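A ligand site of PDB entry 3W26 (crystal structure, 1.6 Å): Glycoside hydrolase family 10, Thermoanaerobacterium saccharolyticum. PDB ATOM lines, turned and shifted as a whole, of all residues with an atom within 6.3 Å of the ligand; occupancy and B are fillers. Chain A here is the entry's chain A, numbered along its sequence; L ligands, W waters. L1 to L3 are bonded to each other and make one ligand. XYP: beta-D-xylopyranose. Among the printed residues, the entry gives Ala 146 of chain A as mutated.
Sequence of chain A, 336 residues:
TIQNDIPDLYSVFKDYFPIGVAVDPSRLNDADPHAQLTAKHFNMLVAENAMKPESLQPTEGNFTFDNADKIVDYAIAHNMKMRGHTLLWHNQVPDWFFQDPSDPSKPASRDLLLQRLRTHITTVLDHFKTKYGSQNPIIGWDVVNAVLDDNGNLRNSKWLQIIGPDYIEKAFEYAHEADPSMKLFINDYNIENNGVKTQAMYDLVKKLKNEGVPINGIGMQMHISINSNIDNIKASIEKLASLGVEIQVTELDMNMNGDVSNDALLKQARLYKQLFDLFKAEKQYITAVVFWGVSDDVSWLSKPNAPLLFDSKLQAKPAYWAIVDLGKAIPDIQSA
Water W2 bridges the side-chain carboxylate of Glu 54 and an oxygen (O1) of XYP L1. Water W9 bridges the indole nitrogen (NE1) of Trp 89 (2.9 Å) and an oxygen (O4) of XYP L3 (3.0 Å).
CZ2 of Trp 89 touches C3 of XYP L3, 3.6 Å away. CD2 of Tyr 189 touches O4 of XYP L3 (3.8 Å). NE2 of His 223 touches C4 of XYP L3 (3.996 Å). CB of Trp 300 touches O3 of XYP L2, at 3.2 Å. Hydrophobic or aromatic side chains within 4 Å of the ligand: His 85, Trp 89, Tyr 189, Trp 292 and Trp 300. Of the 19 residues printed, 13 come within 4 Å of the ligand.
The backbone carbonyl oxygen (O) of Glu 48 is in hydrogen-bond range of the side-chain amino group (NZ) of Lys 52, 3.1 Å away. The backbone carbonyl oxygen of Gln 221 sits close to the backbone NH of Glu 251 (2.9 Å). ND2 of Asn 187 is in hydrogen-bond range of OE1 of Gln 221 (3.2 Å). The side-chain carboxylate of Glu 251 lies within hydrogen-bond range of a ring nitrogen (NE2) of His 223, 2.7 Å away. ND2 of Asn 187 lies within hydrogen-bond range of OE2 of Glu 251 (3.0 Å). The side-chain amide nitrogen (ND2) of Asn 187 lies within hydrogen-bond range of the side-chain amide oxygen (OD1) of Asn 145 (2.9 Å). NZ of Lys 52 lies within hydrogen-bond range of OD1 of Asn 49 (2.9 Å). The side-chain amide oxygen (OE1) of Gln 92 is in hydrogen-bond range of the side-chain amino group (NZ) of Lys 52.
The side-chain carboxylate (OE2) of Glu 48 sits at hydrogen-bond distance from an oxygen (O3) of XYP L2. NE2 of Gln 221 is in hydrogen-bond range of O4 of XYP L3, 2.7 Å away. An oxygen (O2) of XYP L3 sits at hydrogen-bond distance from a ring nitrogen (NE2) of His 85, 2.7 Å away. The side-chain carboxylate (OE2) of Glu 251 sits at hydrogen-bond distance from an oxygen (O3) of XYP L3 (2.8 Å). The side-chain amide nitrogen of Asn 145 is in hydrogen-bond range of an oxygen (O3) of XYP L3 (2.8 Å). An oxygen (O3) of XYP L2 is in hydrogen-bond range of the indole nitrogen (NE1) of Trp 292. NZ of Lys 52 lies close to O2 of XYP L3, 2.9 Å away. The side-chain amide nitrogen (ND2) of Asn 49 is in hydrogen-bond range of an oxygen (O2) of XYP L2. The side-chain amide oxygen (OE1) of Gln 92 lies close to an oxygen (O5) of XYP L2, at 3.2 Å.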
ATOM      1  N   GLU A  48     -10.676  -0.787 -18.539  1.00  0.00           N
ATOM      2  CA  GLU A  48     -10.467   0.404 -19.365  1.00  0.00           C
ATOM      3  C   GLU A  48     -10.678   0.079 -20.836  1.00  0.00           C
ATOM      4  O   GLU A  48     -11.197   0.915 -21.596  1.00  0.00           O
ATOM      5  CB  GLU A  48      -9.056   0.960 -19.143  1.00  0.00           C
ATOM      6  CG  GLU A  48      -8.794   2.271 -19.874  1.00  0.00           C
ATOM      7  CD  GLU A  48      -7.426   2.874 -19.574  1.00  0.00           C
ATOM      8  OE1 GLU A  48      -6.583   2.193 -18.944  1.00  0.00           O
ATOM      9  OE2 GLU A  48      -7.203   4.033 -19.975  1.00  0.00           O
ATOM     10  N   ASN A  49     -10.295  -1.139 -21.244  1.00  0.00           N
ATOM     11  CA  ASN A  49     -10.420  -1.567 -22.640  1.00  0.00           C
ATOM     12  C   ASN A  49     -10.824  -3.018 -22.883  1.00  0.00           C
ATOM     13  O   ASN A  49     -11.385  -3.338 -23.917  1.00  0.00           O
ATOM     14  CB  ASN A  49      -9.095  -1.367 -23.358  1.00  0.00           C
ATOM     15  CG  ASN A  49      -8.761   0.072 -23.550  1.00  0.00           C
ATOM     16  OD1 ASN A  49      -9.446   0.776 -24.294  1.00  0.00           O
ATOM     17  ND2 ASN A  49      -7.712   0.549 -22.883  1.00  0.00           N
ATOM     18  N   LYS A  52     -14.452  -3.927 -24.220  1.00  0.00           N
ATOM     19  CA  LYS A  52     -15.001  -3.213 -25.366  1.00  0.00           C
ATOM     20  C   LYS A  52     -15.286  -4.247 -26.473  1.00  0.00           C
ATOM     21  O   LYS A  52     -14.740  -5.348 -26.481  1.00  0.00           O
ATOM     22  CB  LYS A  52     -14.029  -2.118 -25.827  1.00  0.00           C
ATOM     23  CG  LYS A  52     -14.052  -0.940 -24.869  1.00  0.00           C
ATOM     24  CD  LYS A  52     -12.938   0.085 -25.109  1.00  0.00           C
ATOM     25  CE  LYS A  52     -13.086   1.251 -24.134  1.00  0.00           C
ATOM     26  NZ  LYS A  52     -11.941   2.217 -24.255  1.00  0.00           N
ATOM     27  N   GLU A  54     -14.311  -4.731 -29.651  1.00  0.00           N
ATOM     28  CA  GLU A  54     -13.164  -5.306 -30.369  1.00  0.00           C
ATOM     29  C   GLU A  54     -12.346  -6.212 -29.461  1.00  0.00           C
ATOM     30  O   GLU A  54     -11.708  -7.169 -29.924  1.00  0.00           O
ATOM     31  CB  GLU A  54     -12.243  -4.204 -30.925  1.00  0.00           C
ATOM     32  CG  GLU A  54     -11.495  -3.428 -29.848  1.00  0.00           C
ATOM     33  CD  GLU A  54     -10.455  -2.450 -30.418  1.00  0.00           C
ATOM     34  OE1 GLU A  54     -10.569  -2.076 -31.599  1.00  0.00           O
ATOM     35  OE2 GLU A  54      -9.539  -2.066 -29.669  1.00  0.00           O
ATOM     36  N   HIS A  85     -17.946  -2.248 -19.178  1.00  0.00           N
ATOM     37  CA  HIS A  85     -17.778  -1.205 -20.198  1.00  0.00           C
ATOM     38  C   HIS A  85     -17.158  -1.846 -21.441  1.00  0.00           C
ATOM     39  O   HIS A  85     -16.036  -2.336 -21.363  1.00  0.00           O
ATOM     40  CB  HIS A  85     -16.840  -0.124 -19.646  1.00  0.00           C
ATOM     41  CG  HIS A  85     -16.588   1.021 -20.580  1.00  0.00           C
ATOM     42  ND1 HIS A  85     -17.492   2.042 -20.770  1.00  0.00           N
ATOM     43  CD2 HIS A  85     -15.520   1.305 -21.368  1.00  0.00           C
ATOM     44  CE1 HIS A  85     -16.992   2.908 -21.631  1.00  0.00           C
ATOM     45  NE2 HIS A  85     -15.799   2.492 -22.003  1.00  0.00           N
ATOM     46  N   THR A  86     -17.844  -1.891 -22.583  1.00  0.00           N
ATOM     47  CA  THR A  86     -19.196  -1.364 -22.835  1.00  0.00           C
ATOM     48  C   THR A  86     -19.729  -2.239 -23.987  1.00  0.00           C
ATOM     49  O   THR A  86     -18.945  -2.733 -24.806  1.00  0.00           O
ATOM     50  CB  THR A  86     -19.162   0.138 -23.269  1.00  0.00           C
ATOM     51  OG1 THR A  86     -20.462   0.556 -23.703  1.00  0.00           O
ATOM     52  CG2 THR A  86     -18.156   0.352 -24.405  1.00  0.00           C
ATOM     53  N   TRP A  89     -20.398   0.976 -28.908  1.00  0.00           N
ATOM     54  CA  TRP A  89     -19.689   2.237 -29.021  1.00  0.00           C
ATOM     55  C   TRP A  89     -19.315   2.382 -30.501  1.00  0.00           C
ATOM     56  O   TRP A  89     -19.408   1.406 -31.272  1.00  0.00           O
ATOM     57  CB  TRP A  89     -18.427   2.172 -28.140  1.00  0.00           C
ATOM     58  CG  TRP A  89     -17.696   3.457 -27.931  1.00  0.00           C
ATOM     59  CD1 TRP A  89     -18.210   4.726 -27.932  1.00  0.00           C
ATOM     60  CD2 TRP A  89     -16.303   3.604 -27.594  1.00  0.00           C
ATOM     61  NE1 TRP A  89     -17.233   5.649 -27.622  1.00  0.00           N
ATOM     62  CE2 TRP A  89     -16.056   4.976 -27.408  1.00  0.00           C
ATOM     63  CE3 TRP A  89     -15.244   2.682 -27.433  1.00  0.00           C
ATOM     64  CZ2 TRP A  89     -14.785   5.466 -27.071  1.00  0.00           C
ATOM     65  CZ3 TRP A  89     -13.987   3.178 -27.095  1.00  0.00           C
ATOM     66  CH2 TRP A  89     -13.767   4.561 -26.922  1.00  0.00           C
ATOM     67  N   GLN A  92     -13.402   1.348 -31.141  1.00  0.00           N
ATOM     68  CA  GLN A  92     -13.001   0.030 -30.681  1.00  0.00           C
ATOM     69  C   GLN A  92     -14.083  -1.043 -30.862  1.00  0.00           C
ATOM     70  O   GLN A  92     -14.371  -1.844 -29.966  1.00  0.00           O
ATOM     71  CB  GLN A  92     -12.517   0.102 -29.236  1.00  0.00           C
ATOM     72  CG  GLN A  92     -11.163   0.835 -29.133  1.00  0.00           C
ATOM     73  CD  GLN A  92     -10.707   1.054 -27.710  1.00  0.00           C
ATOM     74  OE1 GLN A  92     -10.929   2.119 -27.125  1.00  0.00           O
ATOM     75  NE2 GLN A  92     -10.056   0.045 -27.132  1.00  0.00           N
ATOM     76  N   ASN A 145     -22.612   3.550 -25.389  1.00  0.00           N
ATOM     77  CA  ASN A 145     -21.625   4.543 -24.995  1.00  0.00           C
ATOM     78  C   ASN A 145     -21.508   5.684 -26.007  1.00  0.00           C
ATOM     79  O   ASN A 145     -21.399   5.436 -27.206  1.00  0.00           O
ATOM     80  CB  ASN A 145     -20.279   3.819 -24.850  1.00  0.00           C
ATOM     81  CG  ASN A 145     -19.260   4.620 -24.063  1.00  0.00           C
ATOM     82  OD1 ASN A 145     -19.579   5.182 -23.018  1.00  0.00           O
ATOM     83  ND2 ASN A 145     -18.012   4.652 -24.551  1.00  0.00           N
ATOM     84  N   ALA A 146     -21.556   6.922 -25.515  1.00  0.00           N
ATOM     85  CA  ALA A 146     -21.378   8.114 -26.351  1.00  0.00           C
ATOM     86  C   ALA A 146     -22.235   8.151 -27.615  1.00  0.00           C
ATOM     87  O   ALA A 146     -21.733   8.425 -28.713  1.00  0.00           O
ATOM     88  CB  ALA A 146     -19.904   8.259 -26.714  1.00  0.00           C
ATOM     89  N   ASN A 187     -24.127   5.773 -21.204  1.00  0.00           N
ATOM     90  CA  ASN A 187     -22.960   6.506 -20.714  1.00  0.00           C
ATOM     91  C   ASN A 187     -22.504   7.575 -21.703  1.00  0.00           C
ATOM     92  O   ASN A 187     -22.517   7.339 -22.914  1.00  0.00           O
ATOM     93  CB  ASN A 187     -21.841   5.466 -20.499  1.00  0.00           C
ATOM     94  CG  ASN A 187     -20.651   6.001 -19.717  1.00  0.00           C
ATOM     95  OD1 ASN A 187     -20.807   6.613 -18.660  1.00  0.00           O
ATOM     96  ND2 ASN A 187     -19.438   5.741 -20.225  1.00  0.00           N
ATOM     97  N   ASP A 188     -22.100   8.740 -21.194  1.00  0.00           N
ATOM     98  CA  ASP A 188     -21.639   9.781 -22.119  1.00  0.00           C
ATOM     99  C   ASP A 188     -20.824  10.874 -21.437  1.00  0.00           C
ATOM    100  O   ASP A 188     -20.878  11.043 -20.214  1.00  0.00           O
ATOM    101  CB  ASP A 188     -22.828  10.423 -22.839  1.00  0.00           C
ATOM    102  CG  ASP A 188     -22.532  10.707 -24.301  1.00  0.00           C
ATOM    103  OD1 ASP A 188     -21.378  11.043 -24.615  1.00  0.00           O
ATOM    104  OD2 ASP A 188     -23.455  10.622 -25.148  1.00  0.00           O
ATOM    105  N   TYR A 189     -20.073  11.604 -22.251  1.00  0.00           N
ATOM    106  CA  TYR A 189     -19.242  12.703 -21.774  1.00  0.00           C
ATOM    107  C   TYR A 189     -19.866  14.042 -22.125  1.00  0.00           C
ATOM    108  O   TYR A 189     -20.730  14.117 -22.999  1.00  0.00           O
ATOM    109  CB  TYR A 189     -17.833  12.611 -22.357  1.00  0.00           C
ATOM    110  CG  TYR A 189     -17.734  12.677 -23.864  1.00  0.00           C
ATOM    111  CD1 TYR A 189     -17.436  13.881 -24.510  1.00  0.00           C
ATOM    112  CD2 TYR A 189     -17.911  11.529 -24.646  1.00  0.00           C
ATOM    113  CE1 TYR A 189     -17.312  13.938 -25.895  1.00  0.00           C
ATOM    114  CE2 TYR A 189     -17.793  11.575 -26.042  1.00  0.00           C
ATOM    115  CZ  TYR A 189     -17.483  12.784 -26.655  1.00  0.00           C
ATOM    116  OH  TYR A 189     -17.341  12.827 -28.017  1.00  0.00           O
ATOM    117  N   GLN A 221     -19.595  10.352 -17.707  1.00  0.00           N
ATOM    118  CA  GLN A 221     -18.162  10.055 -17.767  1.00  0.00           C
ATOM    119  C   GLN A 221     -17.354  10.996 -16.916  1.00  0.00           C
ATOM    120  O   GLN A 221     -16.409  10.580 -16.242  1.00  0.00           O
ATOM    121  CB  GLN A 221     -17.661  10.059 -19.228  1.00  0.00           C
ATOM    122  CG  GLN A 221     -18.260   8.888 -20.026  1.00  0.00           C
ATOM    123  CD  GLN A 221     -17.782   8.785 -21.458  1.00  0.00           C
ATOM    124  OE1 GLN A 221     -18.312   7.969 -22.241  1.00  0.00           O
ATOM    125  NE2 GLN A 221     -16.784   9.573 -21.814  1.00  0.00           N
ATOM    126  N   HIS A 223     -15.284  13.511 -17.758  1.00  0.00           N
ATOM    127  CA  HIS A 223     -13.919  13.787 -18.177  1.00  0.00           C
ATOM    128  C   HIS A 223     -13.903  15.313 -18.134  1.00  0.00           C
ATOM    129  O   HIS A 223     -14.047  15.990 -19.152  1.00  0.00           O
ATOM    130  CB  HIS A 223     -13.671  13.280 -19.591  1.00  0.00           C
ATOM    131  CG  HIS A 223     -13.464  11.799 -19.648  1.00  0.00           C
ATOM    132  ND1 HIS A 223     -12.413  11.177 -19.010  1.00  0.00           N
ATOM    133  CD2 HIS A 223     -14.189  10.821 -20.232  1.00  0.00           C
ATOM    134  CE1 HIS A 223     -12.506   9.869 -19.187  1.00  0.00           C
ATOM    135  NE2 HIS A 223     -13.573   9.623 -19.927  1.00  0.00           N
ATOM    136  N   GLU A 251     -16.060   7.830 -15.450  1.00  0.00           N
ATOM    137  CA  GLU A 251     -14.709   7.895 -16.001  1.00  0.00           C
ATOM    138  C   GLU A 251     -14.042   9.189 -15.576  1.00  0.00           C
ATOM    139  O   GLU A 251     -13.430   9.884 -16.394  1.00  0.00           O
ATOM    140  CB  GLU A 251     -14.792   7.834 -17.535  1.00  0.00           C
ATOM    141  CG  GLU A 251     -15.645   6.683 -18.063  1.00  0.00           C
ATOM    142  CD  GLU A 251     -15.623   6.575 -19.575  1.00  0.00           C
ATOM    143  OE1 GLU A 251     -14.777   7.241 -20.222  1.00  0.00           O
ATOM    144  OE2 GLU A 251     -16.435   5.792 -20.131  1.00  0.00           O
ATOM    145  N   TRP A 292     -10.945   7.253 -14.146  1.00  0.00           N
ATOM    146  CA  TRP A 292     -10.467   6.631 -15.375  1.00  0.00           C
ATOM    147  C   TRP A 292      -8.944   6.486 -15.405  1.00  0.00           C
ATOM    148  O   TRP A 292      -8.238   7.212 -16.122  1.00  0.00           O
ATOM    149  CB  TRP A 292     -10.966   7.433 -16.603  1.00  0.00           C
ATOM    150  CG  TRP A 292     -11.121   6.566 -17.816  1.00  0.00           C
ATOM    151  CD1 TRP A 292     -10.419   6.647 -18.978  1.00  0.00           C
ATOM    152  CD2 TRP A 292     -12.018   5.446 -17.960  1.00  0.00           C
ATOM    153  NE1 TRP A 292     -10.813   5.642 -19.843  1.00  0.00           N
ATOM    154  CE2 TRP A 292     -11.790   4.901 -19.237  1.00  0.00           C
ATOM    155  CE3 TRP A 292     -12.978   4.863 -17.129  1.00  0.00           C
ATOM    156  CZ2 TRP A 292     -12.506   3.777 -19.715  1.00  0.00           C
ATOM    157  CZ3 TRP A 292     -13.687   3.751 -17.596  1.00  0.00           C
ATOM    158  CH2 TRP A 292     -13.443   3.222 -18.872  1.00  0.00           C
ATOM    159  N   SER A 299      -2.562   7.367 -17.398  1.00  0.00           N
ATOM    160  CA  SER A 299      -3.767   8.032 -17.893  1.00  0.00           C
ATOM    161  C   SER A 299      -3.797   8.039 -19.423  1.00  0.00           C
ATOM    162  O   SER A 299      -2.760   8.173 -20.074  1.00  0.00           O
ATOM    163  CB  SER A 299      -3.828   9.472 -17.410  1.00  0.00           C
ATOM    164  OG  SER A 299      -4.869  10.189 -18.064  1.00  0.00           O
ATOM    165  N   TRP A 300      -4.999   7.912 -19.975  1.00  0.00           N
ATOM    166  CA  TRP A 300      -5.190   7.909 -21.430  1.00  0.00           C
ATOM    167  C   TRP A 300      -4.986   9.283 -22.062  1.00  0.00           C
ATOM    168  O   TRP A 300      -4.862   9.383 -23.280  1.00  0.00           O
ATOM    169  CB  TRP A 300      -6.599   7.430 -21.774  1.00  0.00           C
ATOM    170  CG  TRP A 300      -7.695   8.428 -21.438  1.00  0.00           C
ATOM    171  CD1 TRP A 300      -8.016   8.923 -20.207  1.00  0.00           C
ATOM    172  CD2 TRP A 300      -8.608   9.037 -22.362  1.00  0.00           C
ATOM    173  NE1 TRP A 300      -9.077   9.805 -20.314  1.00  0.00           N
ATOM    174  CE2 TRP A 300      -9.456   9.888 -21.622  1.00  0.00           C
ATOM    175  CE3 TRP A 300      -8.786   8.932 -23.751  1.00  0.00           C
ATOM    176  CZ2 TRP A 300     -10.484  10.639 -22.221  1.00  0.00           C
ATOM    177  CZ3 TRP A 300      -9.797   9.686 -24.353  1.00  0.00           C
ATOM    178  CH2 TRP A 300     -10.632  10.527 -23.584  1.00  0.00           C
HETATM  179  O1  XYP L   1      -5.307  -0.218 -29.309  1.00  0.00           O
HETATM  180  C1  XYP L   1      -5.411   0.851 -28.348  1.00  0.00           C
HETATM  181  C2  XYP L   1      -5.733   2.147 -29.075  1.00  0.00           C
HETATM  182  C3  XYP L   1      -5.914   3.261 -28.059  1.00  0.00           C
HETATM  183  C4  XYP L   1      -6.957   2.866 -27.035  1.00  0.00           C
HETATM  184  C5  XYP L   1      -6.538   1.550 -26.395  1.00  0.00           C
HETATM  185  O2  XYP L   1      -4.653   2.476 -29.957  1.00  0.00           O
HETATM  186  O3  XYP L   1      -6.318   4.471 -28.714  1.00  0.00           O
HETATM  187  O4  XYP L   1      -7.012   3.887 -26.035  1.00  0.00           O
HETATM  188  O5  XYP L   1      -6.437   0.526 -27.403  1.00  0.00           O
HETATM  189  C1  XYP L   2      -8.200   3.786 -25.232  1.00  0.00           C
HETATM  190  C2  XYP L   2      -7.867   4.353 -23.869  1.00  0.00           C
HETATM  191  C3  XYP L   2      -9.117   4.399 -23.001  1.00  0.00           C
HETATM  192  C4  XYP L   2     -10.200   5.182 -23.730  1.00  0.00           C
HETATM  193  C5  XYP L   2     -10.443   4.540 -25.076  1.00  0.00           C
HETATM  194  O2  XYP L   2      -6.913   3.488 -23.231  1.00  0.00           O
HETATM  195  O3  XYP L   2      -8.806   5.074 -21.770  1.00  0.00           O
HETATM  196  O4  XYP L   2     -11.398   5.139 -22.946  1.00  0.00           O
HETATM  197  O5  XYP L   2      -9.230   4.567 -25.851  1.00  0.00           O
HETATM  198  C1  XYP L   3     -12.449   5.920 -23.525  1.00  0.00           C
HETATM  199  C2  XYP L   3     -13.770   5.439 -22.948  1.00  0.00           C
HETATM  200  C3  XYP L   3     -14.903   6.262 -23.529  1.00  0.00           C
HETATM  201  C4  XYP L   3     -14.648   7.733 -23.280  1.00  0.00           C
HETATM  202  C5  XYP L   3     -13.280   8.105 -23.832  1.00  0.00           C
HETATM  203  O2  XYP L   3     -13.953   4.052 -23.289  1.00  0.00           O
HETATM  204  O3  XYP L   3     -16.140   5.902 -22.878  1.00  0.00           O
HETATM  205  O4  XYP L   3     -15.645   8.509 -23.970  1.00  0.00           O
HETATM  206  O5  XYP L   3     -12.268   7.303 -23.197  1.00  0.00           O
HETATM  207  O   HOH W   1      -4.545   1.251 -24.512  1.00  0.00           O
HETATM  208  O   HOH W   2      -7.668  -0.375 -30.732  1.00  0.00           O
HETATM  209  O   HOH W   3      -4.195   0.242 -32.070  1.00  0.00           O
HETATM  210  O   HOH W   4      -2.769   4.741 -29.705  1.00  0.00           O
HETATM  211  O   HOH W   5     -12.858   8.517 -26.600  1.00  0.00           O
HETATM  212  O   HOH W   6      -8.515   3.911 -30.108  1.00  0.00           O
HETATM  213  O   HOH W   7      -6.141   6.817 -27.196  1.00  0.00           O
HETATM  214  O   HOH W   8      -4.491   4.609 -23.314  1.00  0.00           O
HETATM  215  O   HOH W   9     -16.540   8.344 -26.810  1.00  0.00           O
HETATM  216  O   HOH W  10      -2.206  -0.767 -27.889  1.00  0.00           O
